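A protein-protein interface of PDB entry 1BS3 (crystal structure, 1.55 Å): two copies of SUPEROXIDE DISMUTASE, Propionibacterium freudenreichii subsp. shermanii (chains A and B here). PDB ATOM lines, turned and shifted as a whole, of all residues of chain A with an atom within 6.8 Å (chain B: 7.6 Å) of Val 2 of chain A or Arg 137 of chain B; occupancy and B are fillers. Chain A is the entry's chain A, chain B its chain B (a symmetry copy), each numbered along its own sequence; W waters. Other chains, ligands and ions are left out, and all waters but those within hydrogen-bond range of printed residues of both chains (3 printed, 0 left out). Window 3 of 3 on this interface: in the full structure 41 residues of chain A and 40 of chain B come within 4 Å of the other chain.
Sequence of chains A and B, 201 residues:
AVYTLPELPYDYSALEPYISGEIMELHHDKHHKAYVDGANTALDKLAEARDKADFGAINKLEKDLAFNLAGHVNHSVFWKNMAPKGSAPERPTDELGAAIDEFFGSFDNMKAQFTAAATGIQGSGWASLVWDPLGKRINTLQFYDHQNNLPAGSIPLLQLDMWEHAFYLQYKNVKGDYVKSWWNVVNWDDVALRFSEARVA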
ATOM      1  N   ALA A   1      20.021  21.188   0.273  1.00  0.00           N
ATOM      2  CA  ALA A   1      21.293  21.241  -0.496  1.00  0.00           C
ATOM      3  C   ALA A   1      21.069  20.705  -1.901  1.00  0.00           C
ATOM      4  O   ALA A   1      20.124  19.951  -2.140  1.00  0.00           O
ATOM      5  CB  ALA A   1      22.366  20.426   0.215  1.00  0.00           C
ATOM      6  N   VAL A   2      21.941  21.089  -2.828  1.00  0.00           N
ATOM      7  CA  VAL A   2      21.819  20.631  -4.205  1.00  0.00           C
ATOM      8  C   VAL A   2      22.146  19.147  -4.294  1.00  0.00           C
ATOM      9  O   VAL A   2      21.398  18.372  -4.887  1.00  0.00           O
ATOM     10  CB  VAL A   2      22.753  21.418  -5.152  1.00  0.00           C
ATOM     11  CG1 VAL A   2      22.658  20.865  -6.570  1.00  0.00           C
ATOM     12  CG2 VAL A   2      22.386  22.894  -5.137  1.00  0.00           C
ATOM     13  N   TYR A   3      23.258  18.761  -3.680  1.00  0.00           N
ATOM     14  CA  TYR A   3      23.698  17.380  -3.693  1.00  0.00           C
ATOM     15  C   TYR A   3      23.522  16.743  -2.331  1.00  0.00           C
ATOM     16  O   TYR A   3      23.720  17.385  -1.301  1.00  0.00           O
ATOM     17  CB  TYR A   3      25.161  17.303  -4.125  1.00  0.00           C
ATOM     18  CG  TYR A   3      25.402  17.913  -5.485  1.00  0.00           C
ATOM     19  CD1 TYR A   3      24.841  17.346  -6.632  1.00  0.00           C
ATOM     20  CD2 TYR A   3      26.174  19.062  -5.625  1.00  0.00           C
ATOM     21  CE1 TYR A   3      25.039  17.910  -7.885  1.00  0.00           C
ATOM     22  CE2 TYR A   3      26.386  19.638  -6.875  1.00  0.00           C
ATOM     23  CZ  TYR A   3      25.813  19.058  -8.002  1.00  0.00           C
ATOM     24  OH  TYR A   3      26.013  19.625  -9.243  1.00  0.00           O
ATOM     25  N   THR A   4      23.120  15.480  -2.337  1.00  0.00           N
ATOM     26  CA  THR A   4      22.912  14.746  -1.099  1.00  0.00           C
ATOM     27  C   THR A   4      23.557  13.377  -1.195  1.00  0.00           C
ATOM     28  O   THR A   4      23.675  12.798  -2.274  1.00  0.00           O
ATOM     29  CB  THR A   4      21.414  14.580  -0.769  1.00  0.00           C
ATOM     30  OG1 THR A   4      20.775  13.846  -1.817  1.00  0.00           O
ATOM     31  CG2 THR A   4      20.741  15.935  -0.621  1.00  0.00           C
ATOM     32  N   VAL A  36      30.300  15.099  -1.657  1.00  0.00           N
ATOM     33  CA  VAL A  36      29.002  15.764  -1.681  1.00  0.00           C
ATOM     34  C   VAL A  36      29.129  17.159  -1.068  1.00  0.00           C
ATOM     35  O   VAL A  36      28.676  18.141  -1.653  1.00  0.00           O
ATOM     36  CB  VAL A  36      27.930  14.944  -0.917  1.00  0.00           C
ATOM     37  CG1 VAL A  36      26.636  15.733  -0.814  1.00  0.00           C
ATOM     38  CG2 VAL A  36      27.685  13.612  -1.624  1.00  0.00           C
ATOM     39  N   ALA A  39      31.184  19.376  -3.395  1.00  0.00           N
ATOM     40  CA  ALA A  39      30.448  19.780  -4.586  1.00  0.00           C
ATOM     41  C   ALA A  39      29.473  20.898  -4.234  1.00  0.00           C
ATOM     42  O   ALA A  39      29.300  21.842  -5.000  1.00  0.00           O
ATOM     43  CB  ALA A  39      29.706  18.590  -5.184  1.00  0.00           C
ATOM     44  N   ASN A  40      28.841  20.789  -3.068  1.00  0.00           N
ATOM     45  CA  ASN A  40      27.895  21.800  -2.618  1.00  0.00           C
ATOM     46  C   ASN A  40      28.599  23.104  -2.310  1.00  0.00           C
ATOM     47  O   ASN A  40      28.090  24.179  -2.625  1.00  0.00           O
ATOM     48  CB  ASN A  40      27.152  21.327  -1.376  1.00  0.00           C
ATOM     49  CG  ASN A  40      26.061  20.339  -1.695  1.00  0.00           C
ATOM     50  OD1 ASN A  40      25.411  20.430  -2.737  1.00  0.00           O
ATOM     51  ND2 ASN A  40      25.841  19.398  -0.794  1.00  0.00           N
ATOM     52  N   LEU A  43      29.508  25.096  -5.470  1.00  0.00           N
ATOM     53  CA  LEU A  43      28.364  25.812  -6.033  1.00  0.00           C
ATOM     54  C   LEU A  43      28.066  27.089  -5.250  1.00  0.00           C
ATOM     55  O   LEU A  43      27.769  28.127  -5.848  1.00  0.00           O
ATOM     56  CB  LEU A  43      27.121  24.916  -6.086  1.00  0.00           C
ATOM     57  CG  LEU A  43      27.132  23.763  -7.098  1.00  0.00           C
ATOM     58  CD1 LEU A  43      25.790  23.051  -7.068  1.00  0.00           C
ATOM     59  CD2 LEU A  43      27.419  24.289  -8.493  1.00  0.00           C
ATOM     60  N   ASP A  44      28.150  27.014  -3.921  1.00  0.00           N
ATOM     61  CA  ASP A  44      27.908  28.176  -3.064  1.00  0.00           C
ATOM     62  C   ASP A  44      28.951  29.254  -3.346  1.00  0.00           C
ATOM     63  O   ASP A  44      28.639  30.446  -3.389  1.00  0.00           O
ATOM     64  CB  ASP A  44      27.982  27.784  -1.581  1.00  0.00           C
ATOM     65  CG  ASP A  44      26.781  26.974  -1.124  1.00  0.00           C
ATOM     66  OD1 ASP A  44      25.721  27.034  -1.786  1.00  0.00           O
ATOM     67  OD2 ASP A  44      26.895  26.283  -0.087  1.00  0.00           O
ATOM     68  N   ARG A  50      29.427  35.259  -8.501  1.00  0.00           N
ATOM     69  CA  ARG A  50      28.530  35.964  -9.412  1.00  0.00           C
ATOM     70  C   ARG A  50      27.920  37.180  -8.729  1.00  0.00           C
ATOM     71  O   ARG A  50      27.802  38.244  -9.336  1.00  0.00           O
ATOM     72  CB  ARG A  50      27.418  35.041  -9.918  1.00  0.00           C
ATOM     73  CG  ARG A  50      27.884  33.968 -10.890  1.00  0.00           C
ATOM     74  CD  ARG A  50      26.701  33.219 -11.498  1.00  0.00           C
ATOM     75  NE  ARG A  50      25.842  32.598 -10.490  1.00  0.00           N
ATOM     76  CZ  ARG A  50      26.001  31.364 -10.017  1.00  0.00           C
ATOM     77  NH1 ARG A  50      26.990  30.594 -10.454  1.00  0.00           N
ATOM     78  NH2 ARG A  50      25.167  30.898  -9.097  1.00  0.00           N
ATOM     79  N   HIS A  72      31.205  12.408  -6.594  1.00  0.00           N
ATOM     80  CA  HIS A  72      29.837  12.124  -6.171  1.00  0.00           C
ATOM     81  C   HIS A  72      29.135  11.234  -7.206  1.00  0.00           C
ATOM     82  O   HIS A  72      28.518  10.235  -6.855  1.00  0.00           O
ATOM     83  CB  HIS A  72      29.079  13.439  -5.967  1.00  0.00           C
ATOM     84  CG  HIS A  72      27.634  13.267  -5.624  1.00  0.00           C
ATOM     85  ND1 HIS A  72      27.161  12.181  -4.916  1.00  0.00           N
ATOM     86  CD2 HIS A  72      26.554  14.037  -5.888  1.00  0.00           C
ATOM     87  CE1 HIS A  72      25.855  12.293  -4.759  1.00  0.00           C
ATOM     88  NE2 HIS A  72      25.461  13.415  -5.342  1.00  0.00           N
ATOM     89  N   ALA B  99      15.867  29.079 -17.366  1.00  0.00           N
ATOM     90  CA  ALA B  99      16.817  28.185 -16.696  1.00  0.00           C
ATOM     91  C   ALA B  99      18.128  28.890 -16.366  1.00  0.00           C
ATOM     92  O   ALA B  99      18.736  28.635 -15.325  1.00  0.00           O
ATOM     93  CB  ALA B  99      17.083  26.960 -17.554  1.00  0.00           C
ATOM     94  N   GLU B 102      17.549  31.107 -13.470  1.00  0.00           N
ATOM     95  CA  GLU B 102      17.407  30.291 -12.275  1.00  0.00           C
ATOM     96  C   GLU B 102      18.748  29.832 -11.721  1.00  0.00           C
ATOM     97  O   GLU B 102      19.015  29.977 -10.527  1.00  0.00           O
ATOM     98  CB  GLU B 102      16.525  29.073 -12.562  1.00  0.00           C
ATOM     99  CG  GLU B 102      16.313  28.180 -11.343  1.00  0.00           C
ATOM    100  CD  GLU B 102      15.441  26.964 -11.619  1.00  0.00           C
ATOM    101  OE1 GLU B 102      15.186  26.643 -12.804  1.00  0.00           O
ATOM    102  OE2 GLU B 102      15.018  26.317 -10.634  1.00  0.00           O
ATOM    103  N   PHE B 103      19.602  29.312 -12.596  1.00  0.00           N
ATOM    104  CA  PHE B 103      20.902  28.803 -12.172  1.00  0.00           C
ATOM    105  C   PHE B 103      22.064  29.799 -12.128  1.00  0.00           C
ATOM    106  O   PHE B 103      23.113  29.490 -11.553  1.00  0.00           O
ATOM    107  CB  PHE B 103      21.274  27.576 -13.010  1.00  0.00           C
ATOM    108  CG  PHE B 103      20.245  26.484 -12.954  1.00  0.00           C
ATOM    109  CD1 PHE B 103      19.870  25.932 -11.730  1.00  0.00           C
ATOM    110  CD2 PHE B 103      19.610  26.045 -14.113  1.00  0.00           C
ATOM    111  CE1 PHE B 103      18.871  24.966 -11.660  1.00  0.00           C
ATOM    112  CE2 PHE B 103      18.608  25.077 -14.057  1.00  0.00           C
ATOM    113  CZ  PHE B 103      18.236  24.537 -12.829  1.00  0.00           C
ATOM    114  N   PHE B 104      21.881  30.992 -12.696  1.00  0.00           N
ATOM    115  CA  PHE B 104      22.951  31.989 -12.706  1.00  0.00           C
ATOM    116  C   PHE B 104      22.547  33.366 -12.196  1.00  0.00           C
ATOM    117  O   PHE B 104      23.403  34.213 -11.958  1.00  0.00           O
ATOM    118  CB  PHE B 104      23.559  32.102 -14.108  1.00  0.00           C
ATOM    119  CG  PHE B 104      24.216  30.838 -14.578  1.00  0.00           C
ATOM    120  CD1 PHE B 104      25.513  30.526 -14.182  1.00  0.00           C
ATOM    121  CD2 PHE B 104      23.521  29.933 -15.374  1.00  0.00           C
ATOM    122  CE1 PHE B 104      26.104  29.325 -14.568  1.00  0.00           C
ATOM    123  CE2 PHE B 104      24.104  28.734 -15.762  1.00  0.00           C
ATOM    124  CZ  PHE B 104      25.396  28.429 -15.360  1.00  0.00           C
ATOM    125  N   VAL B 130      27.025  23.095 -19.262  1.00  0.00           N
ATOM    126  CA  VAL B 130      26.500  21.734 -19.322  1.00  0.00           C
ATOM    127  C   VAL B 130      25.282  21.497 -18.458  1.00  0.00           C
ATOM    128  O   VAL B 130      25.010  22.244 -17.517  1.00  0.00           O
ATOM    129  CB  VAL B 130      27.552  20.681 -18.858  1.00  0.00           C
ATOM    130  CG1 VAL B 130      28.789  20.723 -19.733  1.00  0.00           C
ATOM    131  CG2 VAL B 130      27.920  20.906 -17.395  1.00  0.00           C
ATOM    132  N   TRP B 131      24.551  20.441 -18.799  1.00  0.00           N
ATOM    133  CA  TRP B 131      23.400  20.027 -18.025  1.00  0.00           C
ATOM    134  C   TRP B 131      23.924  18.928 -17.108  1.00  0.00           C
ATOM    135  O   TRP B 131      24.541  17.955 -17.561  1.00  0.00           O
ATOM    136  CB  TRP B 131      22.285  19.463 -18.914  1.00  0.00           C
ATOM    137  CG  TRP B 131      21.158  18.833 -18.119  1.00  0.00           C
ATOM    138  CD1 TRP B 131      20.864  17.499 -18.023  1.00  0.00           C
ATOM    139  CD2 TRP B 131      20.192  19.515 -17.312  1.00  0.00           C
ATOM    140  NE1 TRP B 131      19.775  17.312 -17.206  1.00  0.00           N
ATOM    141  CE2 TRP B 131      19.343  18.531 -16.756  1.00  0.00           C
ATOM    142  CE3 TRP B 131      19.958  20.862 -17.005  1.00  0.00           C
ATOM    143  CZ2 TRP B 131      18.277  18.850 -15.911  1.00  0.00           C
ATOM    144  CZ3 TRP B 131      18.894  21.181 -16.163  1.00  0.00           C
ATOM    145  CH2 TRP B 131      18.068  20.177 -15.627  1.00  0.00           C
ATOM    146  N   ASP B 132      23.722  19.139 -15.814  1.00  0.00           N
ATOM    147  CA  ASP B 132      24.120  18.210 -14.771  1.00  0.00           C
ATOM    148  C   ASP B 132      22.865  17.396 -14.452  1.00  0.00           C
ATOM    149  O   ASP B 132      21.953  17.891 -13.804  1.00  0.00           O
ATOM    150  CB  ASP B 132      24.586  19.018 -13.555  1.00  0.00           C
ATOM    151  CG  ASP B 132      24.645  18.203 -12.272  1.00  0.00           C
ATOM    152  OD1 ASP B 132      24.743  16.958 -12.320  1.00  0.00           O
ATOM    153  OD2 ASP B 132      24.593  18.835 -11.198  1.00  0.00           O
ATOM    154  N   PRO B 133      22.818  16.130 -14.900  1.00  0.00           N
ATOM    155  CA  PRO B 133      21.678  15.229 -14.679  1.00  0.00           C
ATOM    156  C   PRO B 133      21.415  14.901 -13.206  1.00  0.00           C
ATOM    157  O   PRO B 133      20.266  14.715 -12.802  1.00  0.00           O
ATOM    158  CB  PRO B 133      22.081  13.966 -15.448  1.00  0.00           C
ATOM    159  CG  PRO B 133      23.117  14.443 -16.431  1.00  0.00           C
ATOM    160  CD  PRO B 133      23.893  15.431 -15.623  1.00  0.00           C
ATOM    161  N   LEU B 134      22.483  14.800 -12.420  1.00  0.00           N
ATOM    162  CA  LEU B 134      22.373  14.479 -11.002  1.00  0.00           C
ATOM    163  C   LEU B 134      21.751  15.623 -10.209  1.00  0.00           C
ATOM    164  O   LEU B 134      20.787  15.425  -9.471  1.00  0.00           O
ATOM    165  CB  LEU B 134      23.751  14.124 -10.439  1.00  0.00           C
ATOM    166  CG  LEU B 134      23.821  13.577  -9.011  1.00  0.00           C
ATOM    167  CD1 LEU B 134      22.921  12.360  -8.875  1.00  0.00           C
ATOM    168  CD2 LEU B 134      25.258  13.215  -8.677  1.00  0.00           C
ATOM    169  N   GLY B 135      22.303  16.819 -10.366  1.00  0.00           N
ATOM    170  CA  GLY B 135      21.774  17.971  -9.662  1.00  0.00           C
ATOM    171  C   GLY B 135      20.643  18.637 -10.423  1.00  0.00           C
ATOM    172  O   GLY B 135      20.000  19.545  -9.897  1.00  0.00           O
ATOM    173  N   LYS B 136      20.394  18.169 -11.649  1.00  0.00           N
ATOM    174  CA  LYS B 136      19.348  18.713 -12.524  1.00  0.00           C
ATOM    175  C   LYS B 136      19.473  20.225 -12.622  1.00  0.00           C
ATOM    176  O   LYS B 136      18.539  20.969 -12.317  1.00  0.00           O
ATOM    177  CB  LYS B 136      17.957  18.321 -12.024  1.00  0.00           C
ATOM    178  CG  LYS B 136      17.638  16.846 -12.185  1.00  0.00           C
ATOM    179  CD  LYS B 136      16.281  16.519 -11.588  1.00  0.00           C
ATOM    180  CE  LYS B 136      15.936  15.052 -11.779  1.00  0.00           C
ATOM    181  NZ  LYS B 136      14.659  14.675 -11.100  1.00  0.00           N
ATOM    182  N   ARG B 137      20.639  20.672 -13.075  1.00  0.00           N
ATOM    183  CA  ARG B 137      20.919  22.093 -13.190  1.00  0.00           C
ATOM    184  C   ARG B 137      21.930  22.362 -14.290  1.00  0.00           C
ATOM    185  O   ARG B 137      22.527  21.441 -14.839  1.00  0.00           O
ATOM    186  CB  ARG B 137      21.479  22.614 -11.859  1.00  0.00           C
ATOM    187  CG  ARG B 137      22.751  21.890 -11.395  1.00  0.00           C
ATOM    188  CD  ARG B 137      23.260  22.406 -10.053  1.00  0.00           C
ATOM    189  NE  ARG B 137      23.640  23.813 -10.111  1.00  0.00           N
ATOM    190  CZ  ARG B 137      23.057  24.780  -9.409  1.00  0.00           C
ATOM    191  NH1 ARG B 137      22.060  24.500  -8.585  1.00  0.00           N
ATOM    192  NH2 ARG B 137      23.459  26.035  -9.549  1.00  0.00           N
ATOM    193  N   ILE B 138      22.095  23.636 -14.621  1.00  0.00           N
ATOM    194  CA  ILE B 138      23.056  24.036 -15.631  1.00  0.00           C
ATOM    195  C   ILE B 138      24.263  24.579 -14.882  1.00  0.00           C
ATOM    196  O   ILE B 138      24.127  25.445 -14.017  1.00  0.00           O
ATOM    197  CB  ILE B 138      22.510  25.146 -16.548  1.00  0.00           C
ATOM    198  CG1 ILE B 138      21.249  24.671 -17.273  1.00  0.00           C
ATOM    199  CG2 ILE B 138      23.568  25.549 -17.560  1.00  0.00           C
ATOM    200  CD1 ILE B 138      20.622  25.741 -18.149  1.00  0.00           C
ATOM    201  N   ASN B 139      25.435  24.035 -15.188  1.00  0.00           N
ATOM    202  CA  ASN B 139      26.682  24.466 -14.564  1.00  0.00           C
ATOM    203  C   ASN B 139      27.687  24.866 -15.635  1.00  0.00           C
ATOM    204  O   ASN B 139      27.497  24.576 -16.815  1.00  0.00           O
ATOM    205  CB  ASN B 139      27.307  23.308 -13.780  1.00  0.00           C
ATOM    206  CG  ASN B 139      26.532  22.942 -12.530  1.00  0.00           C
ATOM    207  OD1 ASN B 139      25.950  23.804 -11.879  1.00  0.00           O
ATOM    208  ND2 ASN B 139      26.530  21.664 -12.187  1.00  0.00           N
ATOM    209  N   THR B 140      28.722  25.591 -15.233  1.00  0.00           N
ATOM    210  CA  THR B 140      29.793  25.932 -16.159  1.00  0.00           C
ATOM    211  C   THR B 140      30.963  25.067 -15.708  1.00  0.00           C
ATOM    212  O   THR B 140      31.159  24.846 -14.507  1.00  0.00           O
ATOM    213  CB  THR B 140      30.243  27.423 -16.108  1.00  0.00           C
ATOM    214  OG1 THR B 140      30.687  27.761 -14.789  1.00  0.00           O
ATOM    215  CG2 THR B 140      29.118  28.346 -16.535  1.00  0.00           C
ATOM    216  N   ILE B 155      26.209  16.807 -19.851  1.00  0.00           N
ATOM    217  CA  ILE B 155      25.663  17.000 -21.190  1.00  0.00           C
ATOM    218  C   ILE B 155      26.067  18.376 -21.701  1.00  0.00           C
ATOM    219  O   ILE B 155      25.646  19.389 -21.154  1.00  0.00           O
ATOM    220  CB  ILE B 155      24.125  16.920 -21.200  1.00  0.00           C
ATOM    221  CG1 ILE B 155      23.649  15.628 -20.536  1.00  0.00           C
ATOM    222  CG2 ILE B 155      23.611  17.017 -22.635  1.00  0.00           C
ATOM    223  CD1 ILE B 155      24.108  14.378 -21.232  1.00  0.00           C
ATOM    224  N   LEU B 157      25.978  21.732 -23.572  1.00  0.00           N
ATOM    225  CA  LEU B 157      24.941  22.591 -24.136  1.00  0.00           C
ATOM    226  C   LEU B 157      25.555  23.690 -24.994  1.00  0.00           C
ATOM    227  O   LEU B 157      25.068  23.976 -26.087  1.00  0.00           O
ATOM    228  CB  LEU B 157      24.112  23.235 -23.026  1.00  0.00           C
ATOM    229  CG  LEU B 157      23.410  22.321 -22.021  1.00  0.00           C
ATOM    230  CD1 LEU B 157      22.621  23.178 -21.046  1.00  0.00           C
ATOM    231  CD2 LEU B 157      22.495  21.341 -22.737  1.00  0.00           C
ATOM    232  N   PHE B 195      19.273  21.685 -24.616  1.00  0.00           N
ATOM    233  CA  PHE B 195      18.735  21.802 -23.270  1.00  0.00           C
ATOM    234  C   PHE B 195      17.445  20.980 -23.135  1.00  0.00           C
ATOM    235  O   PHE B 195      17.269  20.233 -22.168  1.00  0.00           O
ATOM    236  CB  PHE B 195      18.467  23.273 -22.960  1.00  0.00           C
ATOM    237  CG  PHE B 195      17.892  23.512 -21.602  1.00  0.00           C
ATOM    238  CD1 PHE B 195      18.561  23.072 -20.464  1.00  0.00           C
ATOM    239  CD2 PHE B 195      16.678  24.174 -21.458  1.00  0.00           C
ATOM    240  CE1 PHE B 195      18.027  23.292 -19.201  1.00  0.00           C
ATOM    241  CE2 PHE B 195      16.134  24.400 -20.200  1.00  0.00           C
ATOM    242  CZ  PHE B 195      16.809  23.959 -19.071  1.00  0.00           C
ATOM    243  N   ARG B 199      17.133  17.651 -20.589  1.00  0.00           N
ATOM    244  CA  ARG B 199      16.215  17.566 -19.451  1.00  0.00           C
ATOM    245  C   ARG B 199      15.462  16.238 -19.395  1.00  0.00           C
ATOM    246  O   ARG B 199      15.087  15.776 -18.316  1.00  0.00           O
ATOM    247  CB  ARG B 199      15.197  18.715 -19.482  1.00  0.00           C
ATOM    248  CG  ARG B 199      15.758  20.089 -19.144  1.00  0.00           C
ATOM    249  CD  ARG B 199      14.775  21.207 -19.512  1.00  0.00           C
ATOM    250  NE  ARG B 199      13.832  21.589 -18.453  1.00  0.00           N
ATOM    251  CZ  ARG B 199      14.158  22.233 -17.329  1.00  0.00           C
ATOM    252  NH1 ARG B 199      15.418  22.563 -17.081  1.00  0.00           N
ATOM    253  NH2 ARG B 199      13.214  22.624 -16.480  1.00  0.00           N
HETATM  254  O   HOH W   1      21.089  15.605  -6.529  1.00  0.00           O
HETATM  255  O   HOH W   2      22.751  28.645  -8.838  1.00  0.00           O
HETATM  256  O   HOH W   3      19.322  19.145  -6.928  1.00  0.00           O
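OH of Tyr 3 of chain A lies within hydrogen-bond range of OD2 of Asp 132 of chain B (2.5 Å).
O of Phe 103 of chain B is in hydrogen-bond range of NH2 of Arg 50 of chain A (3.5 Å).
NE of Arg 50 of chain A is in hydrogen-bond range of O of Phe 104 of chain B.
The side-chain amide oxygen (OD1) of Asn 40 of chain A is in hydrogen-bond range of the backbone NH (N) of Tyr 3 of chain A (2.9 Å).
The backbone carbonyl oxygen (O) of Asn 139 of chain B lies within hydrogen-bond range of the backbone NH (N) of Val 130 of chain B, at 2.9 Å.
The side-chain carboxylate of Asp 132 of chain B lies within hydrogen-bond range of the backbone NH of Leu 134 of chain B, 3.1 Å away.
The side-chain carboxylate (OD1) of Asp 132 of chain B lies within hydrogen-bond range of the backbone NH (N) of Gly 135 of chain B, at 3.1 Å.
The backbone NH (N) of Asp 132 of chain B sits at hydrogen-bond distance from the backbone carbonyl oxygen (O) of Arg 137 of chain B.
OD1 of Asn 139 of chain B is in hydrogen-bond range of NE of Arg 137 of chain B, 2.9 Å away.
Among the printed residues, merely in contact across the chains: Val 2 of chain A with Arg 137 of chain B, Tyr 3 of chain A with Gly 135 of chain B, Tyr 3 of chain A with Arg 137 of chain B, Tyr 3 of chain A with Asn 139 of chain B, Leu 43 of chain A with Arg 137 of chain B, Leu 43 of chain A with Asn 139 of chain B and His 72 of chain A with Leu 134 of chain B.
Val 2 of chain A touches one residue of chain B.
Of the printed residues of chain A, Asp 132 of chain B touches Tyr 3 (2.5 Å).
Of the printed residues of chain A, Gly 135 of chain B touches Tyr 3 (3.7 Å).
Of the printed residues of chain A, Arg 137 of chain B touches Val 2, Tyr 3 and Leu 43.
Of the printed residues of chain A, Asn 139 of chain B touches Tyr 3 (3.6 Å) and Leu 43 (3.7 Å).
Ile 155 of chain B touches none of the printed residues of chain A.
The nearest residue of chain B that does not touch Val 2 of chain A is Gly 135 of chain B (4.3 Å).
The nearest printed residue of chain A that does not touch Arg 137 of chain B is Arg 50 of chain A (5.2 Å).
The nearest printed residue of chain B that does not touch Tyr 3 of chain A is Leu 134 of chain B (4.6 Å).
Of the 11 printed residues of chain A, 5 touch a printed residue of chain B.
Hydrophobic or aromatic side chains of chain A within 4 Å of the printed part of chain B: Val 2, Tyr 3, Leu 43 and His 72.
Hydrophobic or aromatic side chains of chain B that line the printed part of chain A: Phe 104 and Leu 134.
Along chain B the printed residues that touch a printed residue of chain A span positions 103 to 139.
Among the printed residues, no Asp or Glu carboxylate lies within 4 Å of a Lys or Arg side-chain nitrogen of the other chain.
No position is printed for both chains.
Water W2 lies within hydrogen-bond range of the guanidinium group of Arg 137 of chain B (2.8 Å), the backbone carbonyl oxygen of Phe 103 of chain B (2.9 Å) and the guanidinium group of Arg 50 of chain A (3.3 Å).
Water W1 lies within hydrogen-bond range of the backbone carbonyl oxygen of Leu 134 of chain B (3.0 Å) and the backbone carbonyl oxygen of Val 2 of chain A (3.2 Å).
Water W3 bridges the backbone carbonyl oxygen (O) of Val 2 of chain A (3.0 Å) and the backbone carbonyl oxygen (O) of Gly 135 of chain B (3.1 Å).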
